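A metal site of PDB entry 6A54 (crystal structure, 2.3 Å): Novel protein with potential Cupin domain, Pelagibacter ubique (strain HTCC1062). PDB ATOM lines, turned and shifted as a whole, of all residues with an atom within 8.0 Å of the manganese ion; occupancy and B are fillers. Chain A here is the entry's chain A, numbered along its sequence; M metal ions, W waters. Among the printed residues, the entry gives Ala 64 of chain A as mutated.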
ATOM      1  N   TYR A  21      12.018 -19.809  18.314  1.00  0.00           N
ATOM      2  CA  TYR A  21      13.354 -19.257  18.084  1.00  0.00           C
ATOM      3  C   TYR A  21      14.476 -20.246  18.459  1.00  0.00           C
ATOM      4  O   TYR A  21      15.166 -20.083  19.464  1.00  0.00           O
ATOM      5  CB  TYR A  21      13.522 -17.945  18.834  1.00  0.00           C
ATOM      6  CG  TYR A  21      12.418 -16.972  18.508  1.00  0.00           C
ATOM      7  CD1 TYR A  21      11.912 -16.887  17.221  1.00  0.00           C
ATOM      8  CD2 TYR A  21      11.843 -16.177  19.491  1.00  0.00           C
ATOM      9  CE1 TYR A  21      10.890 -16.031  16.911  1.00  0.00           C
ATOM     10  CE2 TYR A  21      10.829 -15.305  19.191  1.00  0.00           C
ATOM     11  CZ  TYR A  21      10.349 -15.240  17.895  1.00  0.00           C
ATOM     12  OH  TYR A  21       9.319 -14.367  17.586  1.00  0.00           O
ATOM     13  N   LEU A  53      16.398 -16.193  14.926  1.00  0.00           N
ATOM     14  CA  LEU A  53      15.327 -15.350  15.394  1.00  0.00           C
ATOM     15  C   LEU A  53      14.354 -15.144  14.224  1.00  0.00           C
ATOM     16  O   LEU A  53      14.531 -14.241  13.413  1.00  0.00           O
ATOM     17  CB  LEU A  53      15.879 -14.004  15.860  1.00  0.00           C
ATOM     18  CG  LEU A  53      14.837 -12.916  16.177  1.00  0.00           C
ATOM     19  CD1 LEU A  53      13.780 -13.462  17.115  1.00  0.00           C
ATOM     20  CD2 LEU A  53      15.512 -11.685  16.780  1.00  0.00           C
ATOM     21  N   THR A  54      13.345 -15.992  14.139  1.00  0.00           N
ATOM     22  CA  THR A  54      12.514 -16.055  12.937  1.00  0.00           C
ATOM     23  C   THR A  54      11.621 -14.832  12.706  1.00  0.00           C
ATOM     24  O   THR A  54      11.243 -14.113  13.642  1.00  0.00           O
ATOM     25  CB  THR A  54      11.661 -17.330  12.924  1.00  0.00           C
ATOM     26  OG1 THR A  54      10.848 -17.375  14.101  1.00  0.00           O
ATOM     27  CG2 THR A  54      12.572 -18.577  12.893  1.00  0.00           C
ATOM     28  N   HIS A  56       9.356 -11.909  12.537  1.00  0.00           N
ATOM     29  CA  HIS A  56       8.262 -11.467  13.395  1.00  0.00           C
ATOM     30  C   HIS A  56       8.161  -9.955  13.416  1.00  0.00           C
ATOM     31  O   HIS A  56       8.971  -9.256  12.813  1.00  0.00           O
ATOM     32  CB  HIS A  56       8.463 -11.965  14.832  1.00  0.00           C
ATOM     33  CG  HIS A  56       9.594 -11.279  15.542  1.00  0.00           C
ATOM     34  ND1 HIS A  56      10.879 -11.776  15.524  1.00  0.00           N
ATOM     35  CD2 HIS A  56       9.648 -10.129  16.229  1.00  0.00           C
ATOM     36  CE1 HIS A  56      11.670 -10.972  16.209  1.00  0.00           C
ATOM     37  NE2 HIS A  56      10.944  -9.953  16.651  1.00  0.00           N
ATOM     38  N   TYR A  57       7.142  -9.449  14.109  1.00  0.00           N
ATOM     39  CA  TYR A  57       6.998  -8.028  14.332  1.00  0.00           C
ATOM     40  C   TYR A  57       6.278  -7.791  15.622  1.00  0.00           C
ATOM     41  O   TYR A  57       5.796  -8.725  16.277  1.00  0.00           O
ATOM     42  CB  TYR A  57       6.261  -7.335  13.181  1.00  0.00           C
ATOM     43  CG  TYR A  57       4.818  -7.756  12.992  1.00  0.00           C
ATOM     44  CD1 TYR A  57       4.491  -8.903  12.287  1.00  0.00           C
ATOM     45  CD2 TYR A  57       3.787  -6.976  13.503  1.00  0.00           C
ATOM     46  CE1 TYR A  57       3.185  -9.288  12.118  1.00  0.00           C
ATOM     47  CE2 TYR A  57       2.470  -7.352  13.331  1.00  0.00           C
ATOM     48  CZ  TYR A  57       2.169  -8.508  12.639  1.00  0.00           C
ATOM     49  OH  TYR A  57       0.850  -8.867  12.481  1.00  0.00           O
ATOM     50  N   HIS A  58       6.204  -6.522  15.978  1.00  0.00           N
ATOM     51  CA  HIS A  58       5.470  -6.108  17.153  1.00  0.00           C
ATOM     52  C   HIS A  58       5.294  -4.606  17.054  1.00  0.00           C
ATOM     53  O   HIS A  58       5.921  -3.945  16.218  1.00  0.00           O
ATOM     54  CB  HIS A  58       6.252  -6.494  18.398  1.00  0.00           C
ATOM     55  CG  HIS A  58       7.732  -6.423  18.212  1.00  0.00           C
ATOM     56  ND1 HIS A  58       8.400  -5.231  17.982  1.00  0.00           N
ATOM     57  CD2 HIS A  58       8.681  -7.387  18.218  1.00  0.00           C
ATOM     58  CE1 HIS A  58       9.688  -5.466  17.848  1.00  0.00           C
ATOM     59  NE2 HIS A  58       9.888  -6.775  17.992  1.00  0.00           N
ATOM     60  N   PRO A  60       5.831  -1.850  19.095  1.00  0.00           N
ATOM     61  CA  PRO A  60       6.851  -0.837  19.390  1.00  0.00           C
ATOM     62  C   PRO A  60       8.051  -0.940  18.439  1.00  0.00           C
ATOM     63  O   PRO A  60       8.339  -2.000  17.894  1.00  0.00           O
ATOM     64  CB  PRO A  60       7.298  -1.187  20.818  1.00  0.00           C
ATOM     65  CG  PRO A  60       6.541  -2.462  21.214  1.00  0.00           C
ATOM     66  CD  PRO A  60       5.923  -3.018  19.988  1.00  0.00           C
ATOM     67  N   ALA A  61       8.725   0.194  18.252  1.00  0.00           N
ATOM     68  CA  ALA A  61      10.016   0.226  17.610  1.00  0.00           C
ATOM     69  C   ALA A  61      10.992  -0.545  18.477  1.00  0.00           C
ATOM     70  O   ALA A  61      10.771  -0.712  19.676  1.00  0.00           O
ATOM     71  CB  ALA A  61      10.487   1.647  17.434  1.00  0.00           C
ATOM     72  N   GLU A  62      12.090  -1.003  17.868  1.00  0.00           N
ATOM     73  CA  GLU A  62      13.103  -1.706  18.609  1.00  0.00           C
ATOM     74  C   GLU A  62      14.486  -1.313  18.119  1.00  0.00           C
ATOM     75  O   GLU A  62      14.694  -0.988  16.947  1.00  0.00           O
ATOM     76  CB  GLU A  62      12.890  -3.209  18.493  1.00  0.00           C
ATOM     77  CG  GLU A  62      13.974  -4.073  19.111  1.00  0.00           C
ATOM     78  CD  GLU A  62      13.712  -5.532  18.833  1.00  0.00           C
ATOM     79  OE1 GLU A  62      12.697  -5.815  18.157  1.00  0.00           O
ATOM     80  OE2 GLU A  62      14.500  -6.388  19.270  1.00  0.00           O
ATOM     81  N   ILE A  63      15.434  -1.284  19.040  1.00  0.00           N
ATOM     82  CA  ILE A  63      16.810  -1.109  18.664  1.00  0.00           C
ATOM     83  C   ILE A  63      17.569  -2.333  19.126  1.00  0.00           C
ATOM     84  O   ILE A  63      17.430  -2.782  20.258  1.00  0.00           O
ATOM     85  CB  ILE A  63      17.426   0.165  19.265  1.00  0.00           C
ATOM     86  CG1 ILE A  63      16.914   1.398  18.521  1.00  0.00           C
ATOM     87  CG2 ILE A  63      18.958   0.105  19.235  1.00  0.00           C
ATOM     88  CD1 ILE A  63      17.395   2.711  19.123  1.00  0.00           C
ATOM     89  N   ALA A  64      18.325  -2.900  18.176  1.00  0.00           N
ATOM     90  CA  ALA A  64      19.312  -3.930  18.460  1.00  0.00           C
ATOM     91  C   ALA A  64      20.742  -3.369  18.397  1.00  0.00           C
ATOM     92  O   ALA A  64      21.089  -2.638  17.467  1.00  0.00           O
ATOM     93  CB  ALA A  64      19.171  -5.060  17.483  1.00  0.00           C
ATOM     94  N   ILE A  90      14.516  -1.119  14.162  1.00  0.00           N
ATOM     95  CA  ILE A  90      13.374  -1.848  13.656  1.00  0.00           C
ATOM     96  C   ILE A  90      12.112  -1.102  14.056  1.00  0.00           C
ATOM     97  O   ILE A  90      11.683  -1.197  15.223  1.00  0.00           O
ATOM     98  CB  ILE A  90      13.290  -3.234  14.286  1.00  0.00           C
ATOM     99  CG1 ILE A  90      14.569  -4.018  14.023  1.00  0.00           C
ATOM    100  CG2 ILE A  90      12.062  -3.977  13.765  1.00  0.00           C
ATOM    101  CD1 ILE A  90      14.809  -5.148  15.039  1.00  0.00           C
ATOM    102  N   ALA A  94       7.340  -3.536  11.531  1.00  0.00           N
ATOM    103  CA  ALA A  94       8.292  -4.026  10.540  1.00  0.00           C
ATOM    104  C   ALA A  94       8.739  -5.450  10.828  1.00  0.00           C
ATOM    105  O   ALA A  94       9.240  -5.749  11.915  1.00  0.00           O
ATOM    106  CB  ALA A  94       9.485  -3.094  10.447  1.00  0.00           C
ATOM    107  N   GLU A  95       8.562  -6.330   9.855  1.00  0.00           N
ATOM    108  CA  GLU A  95       8.950  -7.722   9.987  1.00  0.00           C
ATOM    109  C   GLU A  95      10.465  -7.889   9.915  1.00  0.00           C
ATOM    110  O   GLU A  95      11.101  -7.443   8.966  1.00  0.00           O
ATOM    111  CB  GLU A  95       8.274  -8.583   8.923  1.00  0.00           C
ATOM    112  CG  GLU A  95       6.799  -8.827   9.203  1.00  0.00           C
ATOM    113  CD  GLU A  95       6.200  -9.870   8.273  1.00  0.00           C
ATOM    114  OE1 GLU A  95       5.015 -10.191   8.440  1.00  0.00           O
ATOM    115  OE2 GLU A  95       6.917 -10.350   7.377  1.00  0.00           O
ATOM    116  N   HIS A  96      11.036  -8.543  10.917  1.00  0.00           N
ATOM    117  CA  HIS A  96      12.456  -8.772  10.964  1.00  0.00           C
ATOM    118  C   HIS A  96      12.728 -10.150  11.520  1.00  0.00           C
ATOM    119  O   HIS A  96      12.004 -10.625  12.402  1.00  0.00           O
ATOM    120  CB  HIS A  96      13.137  -7.725  11.850  1.00  0.00           C
ATOM    121  CG  HIS A  96      12.506  -7.612  13.200  1.00  0.00           C
ATOM    122  ND1 HIS A  96      11.193  -7.245  13.370  1.00  0.00           N
ATOM    123  CD2 HIS A  96      12.991  -7.861  14.436  1.00  0.00           C
ATOM    124  CE1 HIS A  96      10.897  -7.250  14.654  1.00  0.00           C
ATOM    125  NE2 HIS A  96      11.971  -7.625  15.331  1.00  0.00           N
ATOM    126  N   ALA A  97      13.766 -10.764  10.971  1.00  0.00           N
ATOM    127  CA  ALA A  97      14.357 -11.966  11.521  1.00  0.00           C
ATOM    128  C   ALA A  97      15.879 -11.780  11.537  1.00  0.00           C
ATOM    129  O   ALA A  97      16.420 -10.847  10.919  1.00  0.00           O
ATOM    130  CB  ALA A  97      13.993 -13.169  10.675  1.00  0.00           C
ATOM    131  N   PHE A 108      23.635  -9.868  20.963  1.00  0.00           N
ATOM    132  CA  PHE A 108      23.127  -8.498  20.871  1.00  0.00           C
ATOM    133  C   PHE A 108      22.220  -8.113  22.041  1.00  0.00           C
ATOM    134  O   PHE A 108      21.556  -8.972  22.621  1.00  0.00           O
ATOM    135  CB  PHE A 108      22.378  -8.300  19.556  1.00  0.00           C
ATOM    136  CG  PHE A 108      21.102  -9.105  19.446  1.00  0.00           C
ATOM    137  CD1 PHE A 108      19.903  -8.599  19.923  1.00  0.00           C
ATOM    138  CD2 PHE A 108      21.097 -10.349  18.841  1.00  0.00           C
ATOM    139  CE1 PHE A 108      18.730  -9.323  19.811  1.00  0.00           C
ATOM    140  CE2 PHE A 108      19.917 -11.088  18.719  1.00  0.00           C
ATOM    141  CZ  PHE A 108      18.736 -10.574  19.210  1.00  0.00           C
ATOM    142  N   TRP A 110      18.824  -5.786  22.972  1.00  0.00           N
ATOM    143  CA  TRP A 110      17.722  -5.083  22.334  1.00  0.00           C
ATOM    144  C   TRP A 110      17.143  -4.072  23.310  1.00  0.00           C
ATOM    145  O   TRP A 110      17.334  -4.167  24.512  1.00  0.00           O
ATOM    146  CB  TRP A 110      16.632  -6.042  21.877  1.00  0.00           C
ATOM    147  CG  TRP A 110      15.832  -6.500  23.017  1.00  0.00           C
ATOM    148  CD1 TRP A 110      14.788  -5.849  23.611  1.00  0.00           C
ATOM    149  CD2 TRP A 110      15.998  -7.721  23.743  1.00  0.00           C
ATOM    150  NE1 TRP A 110      14.298  -6.581  24.644  1.00  0.00           N
ATOM    151  CE2 TRP A 110      15.024  -7.737  24.762  1.00  0.00           C
ATOM    152  CE3 TRP A 110      16.877  -8.796  23.636  1.00  0.00           C
ATOM    153  CZ2 TRP A 110      14.895  -8.798  25.655  1.00  0.00           C
ATOM    154  CZ3 TRP A 110      16.751  -9.850  24.535  1.00  0.00           C
ATOM    155  CH2 TRP A 110      15.761  -9.839  25.527  1.00  0.00           C
ATOM    156  N   ILE A 111      16.430  -3.099  22.763  1.00  0.00           N
ATOM    157  CA  ILE A 111      15.772  -2.094  23.557  1.00  0.00           C
ATOM    158  C   ILE A 111      14.411  -1.812  22.972  1.00  0.00           C
ATOM    159  O   ILE A 111      14.239  -1.737  21.749  1.00  0.00           O
ATOM    160  CB  ILE A 111      16.558  -0.764  23.593  1.00  0.00           C
ATOM    161  CG1 ILE A 111      17.946  -0.961  24.227  1.00  0.00           C
ATOM    162  CG2 ILE A 111      15.750   0.310  24.338  1.00  0.00           C
ATOM    163  CD1 ILE A 111      19.020  -1.425  23.225  1.00  0.00           C
ATOM    164  N   PHE A 112      13.434  -1.669  23.858  1.00  0.00           N
ATOM    165  CA  PHE A 112      12.079  -1.274  23.522  1.00  0.00           C
ATOM    166  C   PHE A 112      11.726   0.000  24.337  1.00  0.00           C
ATOM    167  O   PHE A 112      12.214   0.165  25.463  1.00  0.00           O
ATOM    168  CB  PHE A 112      11.108  -2.376  23.932  1.00  0.00           C
ATOM    169  CG  PHE A 112      11.106  -3.589  23.035  1.00  0.00           C
ATOM    170  CD1 PHE A 112      10.660  -3.494  21.729  1.00  0.00           C
ATOM    171  CD2 PHE A 112      11.466  -4.838  23.529  1.00  0.00           C
ATOM    172  CE1 PHE A 112      10.613  -4.629  20.921  1.00  0.00           C
ATOM    173  CE2 PHE A 112      11.429  -5.961  22.715  1.00  0.00           C
ATOM    174  CZ  PHE A 112      11.007  -5.847  21.404  1.00  0.00           C
ATOM    175  N   PHE A 117       9.532  -6.211  29.091  1.00  0.00           N
ATOM    176  CA  PHE A 117       9.518  -7.079  27.927  1.00  0.00           C
ATOM    177  C   PHE A 117       8.131  -7.680  27.695  1.00  0.00           C
ATOM    178  O   PHE A 117       7.698  -7.805  26.548  1.00  0.00           O
ATOM    179  CB  PHE A 117      10.528  -8.216  28.104  1.00  0.00           C
ATOM    180  CG  PHE A 117      10.546  -9.193  26.961  1.00  0.00           C
ATOM    181  CD1 PHE A 117      11.174  -8.874  25.766  1.00  0.00           C
ATOM    182  CD2 PHE A 117       9.937 -10.438  27.093  1.00  0.00           C
ATOM    183  CE1 PHE A 117      11.209  -9.787  24.709  1.00  0.00           C
ATOM    184  CE2 PHE A 117       9.961 -11.363  26.043  1.00  0.00           C
ATOM    185  CZ  PHE A 117      10.590 -11.030  24.845  1.00  0.00           C
ATOM    186  N   VAL A 120       5.212  -6.571  25.625  1.00  0.00           N
ATOM    187  CA  VAL A 120       5.437  -6.526  24.181  1.00  0.00           C
ATOM    188  C   VAL A 120       4.922  -7.786  23.526  1.00  0.00           C
ATOM    189  O   VAL A 120       5.333  -8.886  23.864  1.00  0.00           O
ATOM    190  CB  VAL A 120       6.909  -6.309  23.827  1.00  0.00           C
ATOM    191  CG1 VAL A 120       7.092  -6.432  22.336  1.00  0.00           C
ATOM    192  CG2 VAL A 120       7.356  -4.941  24.298  1.00  0.00           C
ATOM    193  N   TYR A 122       4.167 -10.350  20.540  1.00  0.00           N
ATOM    194  CA  TYR A 122       4.848 -10.812  19.340  1.00  0.00           C
ATOM    195  C   TYR A 122       3.868 -11.379  18.331  1.00  0.00           C
ATOM    196  O   TYR A 122       2.846 -11.980  18.675  1.00  0.00           O
ATOM    197  CB  TYR A 122       5.916 -11.852  19.713  1.00  0.00           C
ATOM    198  CG  TYR A 122       7.270 -11.256  20.054  1.00  0.00           C
ATOM    199  CD1 TYR A 122       7.425 -10.322  21.078  1.00  0.00           C
ATOM    200  CD2 TYR A 122       8.410 -11.668  19.367  1.00  0.00           C
ATOM    201  CE1 TYR A 122       8.697  -9.794  21.386  1.00  0.00           C
ATOM    202  CE2 TYR A 122       9.666 -11.154  19.668  1.00  0.00           C
ATOM    203  CZ  TYR A 122       9.812 -10.215  20.671  1.00  0.00           C
ATOM    204  OH  TYR A 122      11.078  -9.730  20.932  1.00  0.00           O
HETATM  205 MN    MN M   1      11.915  -8.064  17.647  1.00  0.00          MN
HETATM  206  O   HOH W   1      13.861  -9.310  17.924  1.00  0.00           O
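Tyr 122 touches the manganese ion. Within 4 Å of the manganese ion: His 56, His 58, Glu 62, His 96 and Tyr 122. Along chain A the residues within 4 Å of the manganese ion span positions 56 to 122.
ND1 of His 56 lies within hydrogen-bond range of O of Thr 54, at 3.0 Å. ND1 of His 96 is in hydrogen-bond range of O of Ala 94. A ring nitrogen (ND1) of His 58 is in hydrogen-bond range of the backbone carbonyl oxygen of Pro 60. The backbone carbonyl oxygen (O) of Ile 90 lies within hydrogen-bond range of the backbone NH (N) of Glu 62, 2.7 Å away.
The manganese ion is bound by water W1 (2.3 Å), NE2 of His 56 (2.3 Å), NE2 of His 96 (2.4 Å), NE2 of His 58 (2.4 Å) and OE1 of Glu 62 (2.4 Å). The manganese ion has five donor atoms within binding distance.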
